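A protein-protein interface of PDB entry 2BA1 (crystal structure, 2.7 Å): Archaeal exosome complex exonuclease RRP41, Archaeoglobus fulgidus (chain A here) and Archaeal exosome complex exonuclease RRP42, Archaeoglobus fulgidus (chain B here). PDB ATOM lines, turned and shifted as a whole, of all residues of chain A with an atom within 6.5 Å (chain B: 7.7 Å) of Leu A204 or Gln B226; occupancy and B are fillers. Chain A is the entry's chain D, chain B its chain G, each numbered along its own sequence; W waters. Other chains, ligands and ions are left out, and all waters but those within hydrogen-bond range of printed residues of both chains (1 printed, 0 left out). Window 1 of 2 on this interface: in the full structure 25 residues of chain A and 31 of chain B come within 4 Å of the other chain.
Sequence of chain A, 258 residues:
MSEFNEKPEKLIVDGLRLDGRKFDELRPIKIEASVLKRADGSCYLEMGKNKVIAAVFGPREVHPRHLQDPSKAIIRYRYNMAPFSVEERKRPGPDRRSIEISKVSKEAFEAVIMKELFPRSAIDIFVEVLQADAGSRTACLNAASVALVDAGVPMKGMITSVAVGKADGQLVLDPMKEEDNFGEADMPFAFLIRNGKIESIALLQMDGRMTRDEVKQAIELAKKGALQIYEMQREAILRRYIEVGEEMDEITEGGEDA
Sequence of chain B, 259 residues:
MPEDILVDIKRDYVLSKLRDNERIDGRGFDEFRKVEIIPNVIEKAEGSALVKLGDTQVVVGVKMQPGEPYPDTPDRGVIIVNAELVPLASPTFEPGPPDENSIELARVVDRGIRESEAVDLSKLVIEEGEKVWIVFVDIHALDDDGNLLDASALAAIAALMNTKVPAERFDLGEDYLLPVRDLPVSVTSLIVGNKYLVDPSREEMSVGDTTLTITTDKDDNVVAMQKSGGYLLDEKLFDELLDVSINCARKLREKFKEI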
ATOM      1  N   GLU A 100      -9.646   2.206 -14.754  1.00  0.00           N
ATOM      2  CA  GLU A 100      -8.973   0.945 -15.047  1.00  0.00           C
ATOM      3  C   GLU A 100      -7.809   0.708 -14.090  1.00  0.00           C
ATOM      4  O   GLU A 100      -7.686  -0.377 -13.511  1.00  0.00           O
ATOM      5  CB  GLU A 100      -8.456   0.970 -16.482  1.00  0.00           C
ATOM      6  CG  GLU A 100      -8.511  -0.370 -17.185  1.00  0.00           C
ATOM      7  CD  GLU A 100      -7.568  -1.378 -16.580  1.00  0.00           C
ATOM      8  OE1 GLU A 100      -6.346  -1.127 -16.615  1.00  0.00           O
ATOM      9  OE2 GLU A 100      -8.050  -2.415 -16.073  1.00  0.00           O
ATOM     10  N   VAL A 104      -7.545  -2.494 -11.350  1.00  0.00           N
ATOM     11  CA  VAL A 104      -6.445  -3.441 -11.347  1.00  0.00           C
ATOM     12  C   VAL A 104      -5.577  -3.251 -10.104  1.00  0.00           C
ATOM     13  O   VAL A 104      -5.040  -4.225  -9.564  1.00  0.00           O
ATOM     14  CB  VAL A 104      -5.592  -3.307 -12.637  1.00  0.00           C
ATOM     15  CG1 VAL A 104      -5.015  -1.911 -12.751  1.00  0.00           C
ATOM     16  CG2 VAL A 104      -4.502  -4.343 -12.636  1.00  0.00           C
ATOM     17  N   MET A 187       5.316  -2.989 -19.978  1.00  0.00           N
ATOM     18  CA  MET A 187       4.704  -4.030 -19.168  1.00  0.00           C
ATOM     19  C   MET A 187       4.870  -3.898 -17.644  1.00  0.00           C
ATOM     20  O   MET A 187       5.899  -4.273 -17.079  1.00  0.00           O
ATOM     21  CB  MET A 187       5.245  -5.369 -19.642  1.00  0.00           C
ATOM     22  CG  MET A 187       4.747  -6.565 -18.886  1.00  0.00           C
ATOM     23  SD  MET A 187       5.404  -8.030 -19.654  1.00  0.00           S
ATOM     24  CE  MET A 187       4.253  -9.250 -19.051  1.00  0.00           C
ATOM     25  N   PRO A 188       3.848  -3.360 -16.958  1.00  0.00           N
ATOM     26  CA  PRO A 188       3.929  -3.202 -15.503  1.00  0.00           C
ATOM     27  C   PRO A 188       3.544  -4.447 -14.709  1.00  0.00           C
ATOM     28  O   PRO A 188       2.609  -5.152 -15.073  1.00  0.00           O
ATOM     29  CB  PRO A 188       2.986  -2.034 -15.238  1.00  0.00           C
ATOM     30  CG  PRO A 188       1.929  -2.228 -16.279  1.00  0.00           C
ATOM     31  CD  PRO A 188       2.730  -2.566 -17.510  1.00  0.00           C
ATOM     32  N   PHE A 189       4.282  -4.703 -13.627  1.00  0.00           N
ATOM     33  CA  PHE A 189       4.037  -5.842 -12.737  1.00  0.00           C
ATOM     34  C   PHE A 189       3.909  -5.391 -11.288  1.00  0.00           C
ATOM     35  O   PHE A 189       4.126  -4.233 -10.953  1.00  0.00           O
ATOM     36  CB  PHE A 189       5.200  -6.836 -12.710  1.00  0.00           C
ATOM     37  CG  PHE A 189       5.521  -7.471 -14.010  1.00  0.00           C
ATOM     38  CD1 PHE A 189       6.193  -6.763 -14.991  1.00  0.00           C
ATOM     39  CD2 PHE A 189       5.242  -8.820 -14.213  1.00  0.00           C
ATOM     40  CE1 PHE A 189       6.598  -7.388 -16.161  1.00  0.00           C
ATOM     41  CE2 PHE A 189       5.641  -9.462 -15.379  1.00  0.00           C
ATOM     42  CZ  PHE A 189       6.324  -8.742 -16.360  1.00  0.00           C
ATOM     43  N   ALA A 190       3.612  -6.354 -10.431  1.00  0.00           N
ATOM     44  CA  ALA A 190       3.517  -6.137  -9.000  1.00  0.00           C
ATOM     45  C   ALA A 190       3.602  -7.529  -8.403  1.00  0.00           C
ATOM     46  O   ALA A 190       2.951  -8.445  -8.891  1.00  0.00           O
ATOM     47  CB  ALA A 190       2.196  -5.467  -8.630  1.00  0.00           C
ATOM     48  N   ILE A 201       2.648 -13.182  -8.678  1.00  0.00           N
ATOM     49  CA  ILE A 201       2.305 -11.986  -9.434  1.00  0.00           C
ATOM     50  C   ILE A 201       0.975 -11.433  -8.943  1.00  0.00           C
ATOM     51  O   ILE A 201      -0.049 -12.127  -8.943  1.00  0.00           O
ATOM     52  CB  ILE A 201       2.221 -12.284 -10.943  1.00  0.00           C
ATOM     53  CG1 ILE A 201       3.532 -12.924 -11.405  1.00  0.00           C
ATOM     54  CG2 ILE A 201       1.979 -10.997 -11.720  1.00  0.00           C
ATOM     55  CD1 ILE A 201       3.568 -13.289 -12.868  1.00  0.00           C
ATOM     56  N   ALA A 202       1.012 -10.178  -8.504  1.00  0.00           N
ATOM     57  CA  ALA A 202      -0.160  -9.494  -7.993  1.00  0.00           C
ATOM     58  C   ALA A 202      -0.799  -8.642  -9.080  1.00  0.00           C
ATOM     59  O   ALA A 202      -2.021  -8.485  -9.105  1.00  0.00           O
ATOM     60  CB  ALA A 202       0.232  -8.633  -6.822  1.00  0.00           C
ATOM     61  N   LEU A 203       0.022  -8.095  -9.972  1.00  0.00           N
ATOM     62  CA  LEU A 203      -0.489  -7.267 -11.063  1.00  0.00           C
ATOM     63  C   LEU A 203       0.283  -7.482 -12.368  1.00  0.00           C
ATOM     64  O   LEU A 203       1.506  -7.381 -12.396  1.00  0.00           O
ATOM     65  CB  LEU A 203      -0.459  -5.781 -10.662  1.00  0.00           C
ATOM     66  CG  LEU A 203      -0.956  -4.746 -11.682  1.00  0.00           C
ATOM     67  CD1 LEU A 203      -1.486  -3.542 -10.938  1.00  0.00           C
ATOM     68  CD2 LEU A 203       0.145  -4.320 -12.636  1.00  0.00           C
ATOM     69  N   LEU A 204      -0.431  -7.765 -13.455  1.00  0.00           N
ATOM     70  CA  LEU A 204       0.228  -8.000 -14.735  1.00  0.00           C
ATOM     71  C   LEU A 204      -0.549  -7.395 -15.894  1.00  0.00           C
ATOM     72  O   LEU A 204      -1.734  -7.654 -16.038  1.00  0.00           O
ATOM     73  CB  LEU A 204       0.390  -9.510 -14.958  1.00  0.00           C
ATOM     74  CG  LEU A 204       1.410 -10.024 -15.981  1.00  0.00           C
ATOM     75  CD1 LEU A 204       1.591 -11.515 -15.804  1.00  0.00           C
ATOM     76  CD2 LEU A 204       0.959  -9.723 -17.385  1.00  0.00           C
ATOM     77  N   GLN A 205       0.134  -6.599 -16.715  1.00  0.00           N
ATOM     78  CA  GLN A 205      -0.458  -5.952 -17.894  1.00  0.00           C
ATOM     79  C   GLN A 205       0.622  -5.710 -18.956  1.00  0.00           C
ATOM     80  O   GLN A 205       1.727  -5.296 -18.614  1.00  0.00           O
ATOM     81  CB  GLN A 205      -1.061  -4.587 -17.535  1.00  0.00           C
ATOM     82  CG  GLN A 205      -2.326  -4.585 -16.708  1.00  0.00           C
ATOM     83  CD  GLN A 205      -2.809  -3.160 -16.439  1.00  0.00           C
ATOM     84  OE1 GLN A 205      -2.225  -2.429 -15.625  1.00  0.00           O
ATOM     85  NE2 GLN A 205      -3.867  -2.753 -17.139  1.00  0.00           N
ATOM     86  N   MET A 206       0.313  -5.940 -20.234  1.00  0.00           N
ATOM     87  CA  MET A 206       1.295  -5.690 -21.291  1.00  0.00           C
ATOM     88  C   MET A 206       0.694  -5.031 -22.529  1.00  0.00           C
ATOM     89  O   MET A 206      -0.446  -5.279 -22.891  1.00  0.00           O
ATOM     90  CB  MET A 206       2.023  -6.993 -21.683  1.00  0.00           C
ATOM     91  CG  MET A 206       1.660  -7.622 -23.047  1.00  0.00           C
ATOM     92  SD  MET A 206       2.345  -6.820 -24.557  1.00  0.00           S
ATOM     93  CE  MET A 206       3.842  -7.679 -24.747  1.00  0.00           C
ATOM     94  N   ILE A 219       9.811 -10.931 -16.955  1.00  0.00           N
ATOM     95  CA  ILE A 219       9.484 -11.180 -15.561  1.00  0.00           C
ATOM     96  C   ILE A 219      10.767 -11.156 -14.741  1.00  0.00           C
ATOM     97  O   ILE A 219      10.793 -10.653 -13.614  1.00  0.00           O
ATOM     98  CB  ILE A 219       8.817 -12.557 -15.347  1.00  0.00           C
ATOM     99  CG1 ILE A 219       7.471 -12.626 -16.061  1.00  0.00           C
ATOM    100  CG2 ILE A 219       8.597 -12.802 -13.875  1.00  0.00           C
ATOM    101  CD1 ILE A 219       7.555 -13.201 -17.450  1.00  0.00           C
ATOM    102  N   GLU B 104     -12.968  -2.029 -19.123  1.00  0.00           N
ATOM    103  CA  GLU B 104     -11.844  -2.951 -19.214  1.00  0.00           C
ATOM    104  C   GLU B 104     -11.935  -3.838 -20.458  1.00  0.00           C
ATOM    105  O   GLU B 104     -10.935  -4.054 -21.160  1.00  0.00           O
ATOM    106  CB  GLU B 104     -11.784  -3.822 -17.956  1.00  0.00           C
ATOM    107  CG  GLU B 104     -10.392  -4.339 -17.637  1.00  0.00           C
ATOM    108  CD  GLU B 104     -10.353  -5.168 -16.368  1.00  0.00           C
ATOM    109  OE1 GLU B 104      -9.240  -5.410 -15.847  1.00  0.00           O
ATOM    110  OE2 GLU B 104     -11.433  -5.585 -15.891  1.00  0.00           O
ATOM    111  N   ARG B 107     -11.181  -1.694 -23.504  1.00  0.00           N
ATOM    112  CA  ARG B 107      -9.764  -1.382 -23.564  1.00  0.00           C
ATOM    113  C   ARG B 107      -8.932  -2.574 -23.995  1.00  0.00           C
ATOM    114  O   ARG B 107      -8.011  -2.421 -24.786  1.00  0.00           O
ATOM    115  CB  ARG B 107      -9.252  -0.846 -22.218  1.00  0.00           C
ATOM    116  CG  ARG B 107      -9.764   0.532 -21.855  1.00  0.00           C
ATOM    117  CD  ARG B 107      -8.948   1.127 -20.721  1.00  0.00           C
ATOM    118  NE  ARG B 107      -8.113   2.254 -21.151  1.00  0.00           N
ATOM    119  CZ  ARG B 107      -6.890   2.492 -20.691  1.00  0.00           C
ATOM    120  NH1 ARG B 107      -6.202   3.538 -21.128  1.00  0.00           N
ATOM    121  NH2 ARG B 107      -6.344   1.666 -19.805  1.00  0.00           N
ATOM    122  N   VAL B 108      -9.234  -3.763 -23.482  1.00  0.00           N
ATOM    123  CA  VAL B 108      -8.462  -4.934 -23.894  1.00  0.00           C
ATOM    124  C   VAL B 108      -8.604  -5.137 -25.408  1.00  0.00           C
ATOM    125  O   VAL B 108      -7.628  -5.050 -26.150  1.00  0.00           O
ATOM    126  CB  VAL B 108      -8.919  -6.222 -23.164  1.00  0.00           C
ATOM    127  CG1 VAL B 108      -8.195  -7.427 -23.731  1.00  0.00           C
ATOM    128  CG2 VAL B 108      -8.636  -6.101 -21.693  1.00  0.00           C
ATOM    129  N   ARG B 111      -6.656  -2.606 -27.197  1.00  0.00           N
ATOM    130  CA  ARG B 111      -5.217  -2.816 -27.174  1.00  0.00           C
ATOM    131  C   ARG B 111      -4.739  -3.869 -28.167  1.00  0.00           C
ATOM    132  O   ARG B 111      -3.701  -3.690 -28.813  1.00  0.00           O
ATOM    133  CB  ARG B 111      -4.777  -3.179 -25.754  1.00  0.00           C
ATOM    134  CG  ARG B 111      -4.839  -2.000 -24.779  1.00  0.00           C
ATOM    135  CD  ARG B 111      -5.268  -2.452 -23.380  1.00  0.00           C
ATOM    136  NE  ARG B 111      -4.246  -3.232 -22.682  1.00  0.00           N
ATOM    137  CZ  ARG B 111      -4.488  -3.970 -21.603  1.00  0.00           C
ATOM    138  NH1 ARG B 111      -3.513  -4.648 -21.021  1.00  0.00           N
ATOM    139  NH2 ARG B 111      -5.714  -4.047 -21.111  1.00  0.00           N
ATOM    140  N   LEU B 149     -15.175 -11.334 -23.403  1.00  0.00           N
ATOM    141  CA  LEU B 149     -13.938 -10.748 -23.909  1.00  0.00           C
ATOM    142  C   LEU B 149     -13.460 -11.394 -25.201  1.00  0.00           C
ATOM    143  O   LEU B 149     -13.453 -10.760 -26.255  1.00  0.00           O
ATOM    144  CB  LEU B 149     -12.849 -10.839 -22.832  1.00  0.00           C
ATOM    145  CG  LEU B 149     -11.415 -10.373 -23.116  1.00  0.00           C
ATOM    146  CD1 LEU B 149     -11.386  -8.977 -23.733  1.00  0.00           C
ATOM    147  CD2 LEU B 149     -10.650 -10.400 -21.807  1.00  0.00           C
ATOM    148  N   VAL B 187      -7.042 -14.834 -25.562  1.00  0.00           N
ATOM    149  CA  VAL B 187      -7.436 -16.088 -24.934  1.00  0.00           C
ATOM    150  C   VAL B 187      -7.514 -15.811 -23.451  1.00  0.00           C
ATOM    151  O   VAL B 187      -6.494 -15.532 -22.820  1.00  0.00           O
ATOM    152  CB  VAL B 187      -6.373 -17.201 -25.139  1.00  0.00           C
ATOM    153  CG1 VAL B 187      -6.774 -18.444 -24.367  1.00  0.00           C
ATOM    154  CG2 VAL B 187      -6.222 -17.526 -26.617  1.00  0.00           C
ATOM    155  N   THR B 188      -8.719 -15.877 -22.897  1.00  0.00           N
ATOM    156  CA  THR B 188      -8.893 -15.640 -21.474  1.00  0.00           C
ATOM    157  C   THR B 188      -9.059 -16.969 -20.769  1.00  0.00           C
ATOM    158  O   THR B 188      -9.754 -17.859 -21.248  1.00  0.00           O
ATOM    159  CB  THR B 188     -10.123 -14.766 -21.183  1.00  0.00           C
ATOM    160  OG1 THR B 188     -10.045 -13.563 -21.956  1.00  0.00           O
ATOM    161  CG2 THR B 188     -10.159 -14.392 -19.708  1.00  0.00           C
ATOM    162  N   SER B 189      -8.412 -17.099 -19.624  1.00  0.00           N
ATOM    163  CA  SER B 189      -8.478 -18.329 -18.861  1.00  0.00           C
ATOM    164  C   SER B 189      -8.849 -17.946 -17.450  1.00  0.00           C
ATOM    165  O   SER B 189      -8.515 -16.845 -16.999  1.00  0.00           O
ATOM    166  CB  SER B 189      -7.109 -19.023 -18.852  1.00  0.00           C
ATOM    167  OG  SER B 189      -6.397 -18.788 -20.064  1.00  0.00           O
ATOM    168  N   THR B 211      -9.036 -13.990 -13.594  1.00  0.00           N
ATOM    169  CA  THR B 211      -8.622 -14.433 -14.916  1.00  0.00           C
ATOM    170  C   THR B 211      -7.298 -13.865 -15.410  1.00  0.00           C
ATOM    171  O   THR B 211      -6.739 -12.949 -14.822  1.00  0.00           O
ATOM    172  CB  THR B 211      -9.692 -14.080 -15.989  1.00  0.00           C
ATOM    173  OG1 THR B 211      -9.604 -12.687 -16.325  1.00  0.00           O
ATOM    174  CG2 THR B 211     -11.093 -14.393 -15.476  1.00  0.00           C
ATOM    175  N   LEU B 212      -6.822 -14.435 -16.515  1.00  0.00           N
ATOM    176  CA  LEU B 212      -5.588 -14.030 -17.173  1.00  0.00           C
ATOM    177  C   LEU B 212      -5.976 -14.025 -18.652  1.00  0.00           C
ATOM    178  O   LEU B 212      -6.678 -14.910 -19.120  1.00  0.00           O
ATOM    179  CB  LEU B 212      -4.462 -15.041 -16.873  1.00  0.00           C
ATOM    180  CG  LEU B 212      -3.013 -14.756 -17.311  1.00  0.00           C
ATOM    181  CD1 LEU B 212      -2.813 -15.156 -18.741  1.00  0.00           C
ATOM    182  CD2 LEU B 212      -2.685 -13.279 -17.133  1.00  0.00           C
ATOM    183  N   THR B 213      -5.542 -13.005 -19.371  1.00  0.00           N
ATOM    184  CA  THR B 213      -5.884 -12.837 -20.765  1.00  0.00           C
ATOM    185  C   THR B 213      -4.621 -12.522 -21.548  1.00  0.00           C
ATOM    186  O   THR B 213      -3.878 -11.595 -21.207  1.00  0.00           O
ATOM    187  CB  THR B 213      -6.887 -11.659 -20.922  1.00  0.00           C
ATOM    188  OG1 THR B 213      -8.050 -11.918 -20.131  1.00  0.00           O
ATOM    189  CG2 THR B 213      -7.300 -11.479 -22.356  1.00  0.00           C
ATOM    190  N   ILE B 214      -4.373 -13.290 -22.602  1.00  0.00           N
ATOM    191  CA  ILE B 214      -3.197 -13.062 -23.421  1.00  0.00           C
ATOM    192  C   ILE B 214      -3.660 -12.890 -24.847  1.00  0.00           C
ATOM    193  O   ILE B 214      -4.433 -13.696 -25.354  1.00  0.00           O
ATOM    194  CB  ILE B 214      -2.200 -14.253 -23.324  1.00  0.00           C
ATOM    195  CG1 ILE B 214      -1.905 -14.555 -21.850  1.00  0.00           C
ATOM    196  CG2 ILE B 214      -0.907 -13.919 -24.072  1.00  0.00           C
ATOM    197  CD1 ILE B 214      -0.910 -15.666 -21.614  1.00  0.00           C
ATOM    198  N   THR B 215      -3.199 -11.830 -25.491  1.00  0.00           N
ATOM    199  CA  THR B 215      -3.572 -11.564 -26.866  1.00  0.00           C
ATOM    200  C   THR B 215      -2.342 -11.749 -27.735  1.00  0.00           C
ATOM    201  O   THR B 215      -1.261 -11.256 -27.413  1.00  0.00           O
ATOM    202  CB  THR B 215      -4.119 -10.124 -27.035  1.00  0.00           C
ATOM    203  OG1 THR B 215      -5.375 -10.003 -26.358  1.00  0.00           O
ATOM    204  CG2 THR B 215      -4.318  -9.790 -28.505  1.00  0.00           C
ATOM    205  N   VAL B 222       3.103 -11.841 -28.500  1.00  0.00           N
ATOM    206  CA  VAL B 222       2.185 -11.298 -27.511  1.00  0.00           C
ATOM    207  C   VAL B 222       2.066  -9.800 -27.742  1.00  0.00           C
ATOM    208  O   VAL B 222       3.043  -9.045 -27.641  1.00  0.00           O
ATOM    209  CB  VAL B 222       2.673 -11.561 -26.086  1.00  0.00           C
ATOM    210  CG1 VAL B 222       1.674 -11.015 -25.102  1.00  0.00           C
ATOM    211  CG2 VAL B 222       2.854 -13.054 -25.874  1.00  0.00           C
ATOM    212  N   ALA B 224      -0.576  -8.111 -26.206  1.00  0.00           N
ATOM    213  CA  ALA B 224      -1.164  -7.572 -24.990  1.00  0.00           C
ATOM    214  C   ALA B 224      -1.541  -8.647 -23.982  1.00  0.00           C
ATOM    215  O   ALA B 224      -1.901  -9.761 -24.346  1.00  0.00           O
ATOM    216  CB  ALA B 224      -2.387  -6.738 -25.334  1.00  0.00           C
ATOM    217  N   MET B 225      -1.456  -8.297 -22.704  1.00  0.00           N
ATOM    218  CA  MET B 225      -1.805  -9.218 -21.628  1.00  0.00           C
ATOM    219  C   MET B 225      -2.593  -8.491 -20.538  1.00  0.00           C
ATOM    220  O   MET B 225      -2.529  -7.266 -20.433  1.00  0.00           O
ATOM    221  CB  MET B 225      -0.542  -9.819 -21.023  1.00  0.00           C
ATOM    222  CG  MET B 225       0.345 -10.531 -22.018  1.00  0.00           C
ATOM    223  SD  MET B 225       1.557 -11.548 -21.173  1.00  0.00           S
ATOM    224  CE  MET B 225       0.452 -12.689 -20.391  1.00  0.00           C
ATOM    225  N   GLN B 226      -3.321  -9.247 -19.720  1.00  0.00           N
ATOM    226  CA  GLN B 226      -4.124  -8.651 -18.657  1.00  0.00           C
ATOM    227  C   GLN B 226      -4.624  -9.674 -17.635  1.00  0.00           C
ATOM    228  O   GLN B 226      -5.332 -10.605 -17.983  1.00  0.00           O
ATOM    229  CB  GLN B 226      -5.326  -7.911 -19.288  1.00  0.00           C
ATOM    230  CG  GLN B 226      -6.356  -7.278 -18.323  1.00  0.00           C
ATOM    231  CD  GLN B 226      -5.865  -5.987 -17.699  1.00  0.00           C
ATOM    232  OE1 GLN B 226      -5.027  -5.296 -18.279  1.00  0.00           O
ATOM    233  N   LYS B 227      -4.242  -9.517 -16.375  1.00  0.00           N
ATOM    234  CA  LYS B 227      -4.746 -10.419 -15.352  1.00  0.00           C
ATOM    235  C   LYS B 227      -5.657  -9.562 -14.500  1.00  0.00           C
ATOM    236  O   LYS B 227      -5.240  -8.525 -13.995  1.00  0.00           O
ATOM    237  CB  LYS B 227      -3.616 -11.045 -14.515  1.00  0.00           C
ATOM    238  CG  LYS B 227      -2.647 -10.120 -13.828  1.00  0.00           C
ATOM    239  CD  LYS B 227      -2.949 -10.026 -12.332  1.00  0.00           C
ATOM    240  CE  LYS B 227      -2.889 -11.371 -11.606  1.00  0.00           C
ATOM    241  NZ  LYS B 227      -3.271 -11.211 -10.159  1.00  0.00           N
ATOM    242  N   SER B 228      -6.912  -9.975 -14.373  1.00  0.00           N
ATOM    243  CA  SER B 228      -7.888  -9.219 -13.596  1.00  0.00           C
ATOM    244  C   SER B 228      -8.440 -10.076 -12.472  1.00  0.00           C
ATOM    245  O   SER B 228      -8.560 -11.284 -12.621  1.00  0.00           O
ATOM    246  CB  SER B 228      -9.030  -8.755 -14.506  1.00  0.00           C
ATOM    247  N   GLY B 229      -8.761  -9.450 -11.345  1.00  0.00           N
ATOM    248  CA  GLY B 229      -9.308 -10.184 -10.218  1.00  0.00           C
ATOM    249  C   GLY B 229      -8.413 -10.178  -8.997  1.00  0.00           C
ATOM    250  O   GLY B 229      -7.210  -9.928  -9.102  1.00  0.00           O
ATOM    251  N   TYR B 231      -6.484 -12.052  -7.002  1.00  0.00           N
ATOM    252  CA  TYR B 231      -5.777 -13.310  -6.813  1.00  0.00           C
ATOM    253  C   TYR B 231      -4.299 -13.206  -7.185  1.00  0.00           C
ATOM    254  O   TYR B 231      -3.896 -12.341  -7.976  1.00  0.00           O
ATOM    255  CB  TYR B 231      -6.434 -14.409  -7.651  1.00  0.00           C
ATOM    256  CG  TYR B 231      -6.036 -14.361  -9.106  1.00  0.00           C
ATOM    257  CD1 TYR B 231      -5.127 -15.280  -9.627  1.00  0.00           C
ATOM    258  CD2 TYR B 231      -6.541 -13.379  -9.957  1.00  0.00           C
ATOM    259  CE1 TYR B 231      -4.732 -15.225 -10.961  1.00  0.00           C
ATOM    260  CE2 TYR B 231      -6.152 -13.314 -11.291  1.00  0.00           C
ATOM    261  CZ  TYR B 231      -5.245 -14.243 -11.785  1.00  0.00           C
ATOM    262  OH  TYR B 231      -4.855 -14.189 -13.103  1.00  0.00           O
ATOM    263  N   LEU B 233      -1.081 -14.737  -9.009  1.00  0.00           N
ATOM    264  CA  LEU B 233      -0.724 -15.591 -10.140  1.00  0.00           C
ATOM    265  C   LEU B 233       0.603 -16.292  -9.871  1.00  0.00           C
ATOM    266  O   LEU B 233       1.618 -15.642  -9.609  1.00  0.00           O
ATOM    267  CB  LEU B 233      -0.577 -14.764 -11.418  1.00  0.00           C
ATOM    268  CG  LEU B 233      -1.129 -15.275 -12.759  1.00  0.00           C
ATOM    269  CD1 LEU B 233      -0.312 -14.632 -13.883  1.00  0.00           C
ATOM    270  CD2 LEU B 233      -1.064 -16.786 -12.867  1.00  0.00           C
ATOM    271  N   PHE B 238       1.826 -19.305 -14.957  1.00  0.00           N
ATOM    272  CA  PHE B 238       1.870 -18.302 -16.003  1.00  0.00           C
ATOM    273  C   PHE B 238       2.658 -18.773 -17.221  1.00  0.00           C
ATOM    274  O   PHE B 238       2.121 -18.812 -18.326  1.00  0.00           O
ATOM    275  CB  PHE B 238       2.471 -17.004 -15.468  1.00  0.00           C
ATOM    276  CG  PHE B 238       2.659 -15.959 -16.516  1.00  0.00           C
ATOM    277  CD1 PHE B 238       1.572 -15.465 -17.216  1.00  0.00           C
ATOM    278  CD2 PHE B 238       3.929 -15.485 -16.822  1.00  0.00           C
ATOM    279  CE1 PHE B 238       1.736 -14.510 -18.209  1.00  0.00           C
ATOM    280  CE2 PHE B 238       4.111 -14.527 -17.817  1.00  0.00           C
ATOM    281  CZ  PHE B 238       3.005 -14.037 -18.516  1.00  0.00           C
HETATM  282  O   HOH W   1      -3.066  -7.033 -13.306  1.00  0.00           O
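The backbone carbonyl oxygen (O) of Ile A201 is in hydrogen-bond range of the backbone NH (N) of Leu B233. O of Ala A202 is in hydrogen-bond range of NZ of Lys B227 (3.2 Å). The backbone carbonyl oxygen (O) of Leu A204 sits at hydrogen-bond distance from the backbone NH (N) of Lys B227. The side-chain amide nitrogen of Gln A205 is in hydrogen-bond range of the side-chain amide oxygen of Gln B226, 3.0 Å away. SD of Met A206 sits at hydrogen-bond distance from N of Ala B224 (3.6 Å). N of Met A206 lies within hydrogen-bond range of O of Met B225, at 3.1 Å. The side-chain carboxylate of Glu B104 sits close to the side-chain carboxylate of Glu A100, 3.2 Å away.
Hydrophobic or aromatic side chains of chain B within 4 Å of the printed part of chain A: Val B222, Ala B224, Met B225, Leu B233 and Phe B238. Among the printed residues, 18 pairs touch across the chains.
CD of Arg B107 touches CG of Glu A100 (3.9 Å). Lys B227 touches Ile A201 (NZ to O, 3.6 Å). Leu A203 touches Lys B227. CD2 of Leu A204 touches CB of Met B225 (3.9 Å). CA of Gln B226 touches O of Leu A204 (3.7 Å). CE1 of Phe B238 touches CD1 of Leu A204 (3.8 Å). Gln A205 touches Met B225. NH1 of Arg B111 touches O of Met A206, at 3.6 Å. Met A206 touches Val B222. CE2 of Phe B238 touches CD1 of Ile A219, 3.7 Å away.
Water W1 bridges O of Lys B227 and N of Leu A204.
Leu A204 touches just these residues of chain B: Met B225, Gln B226, Lys B227 and Phe B238. Of the printed residues of chain B, Ile A219 touches Phe B238 (3.7 Å). Of the printed residues of chain A, Glu B104 touches Glu A100. Of the printed residues of chain A, Arg B107 touches Glu A100 (3.9 Å). Leu B149 touches none of the printed residues of chain A. Printed residues of chain A within 4 Å of Ala B224: Met A206. Gln B226 touches two residues of chain A.
The backbone carbonyl oxygen of Pro A188 sits at hydrogen-bond distance from the backbone NH of Gln A205 (3.3 Å). O of Ala A190 is in hydrogen-bond range of N of Ala A202, 2.6 Å away. N of Ala A190 is in hydrogen-bond range of O of Leu A203, at 3.1 Å. O of Met B225 sits at hydrogen-bond distance from NH1 of Arg B111, 2.9 Å away. The backbone carbonyl oxygen of Thr B211 lies within hydrogen-bond range of the side-chain hydroxyl of Tyr B231 (2.8 Å). The backbone NH (N) of Thr B215 is in hydrogen-bond range of the backbone carbonyl oxygen (O) of Ala B224, at 2.7 Å.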
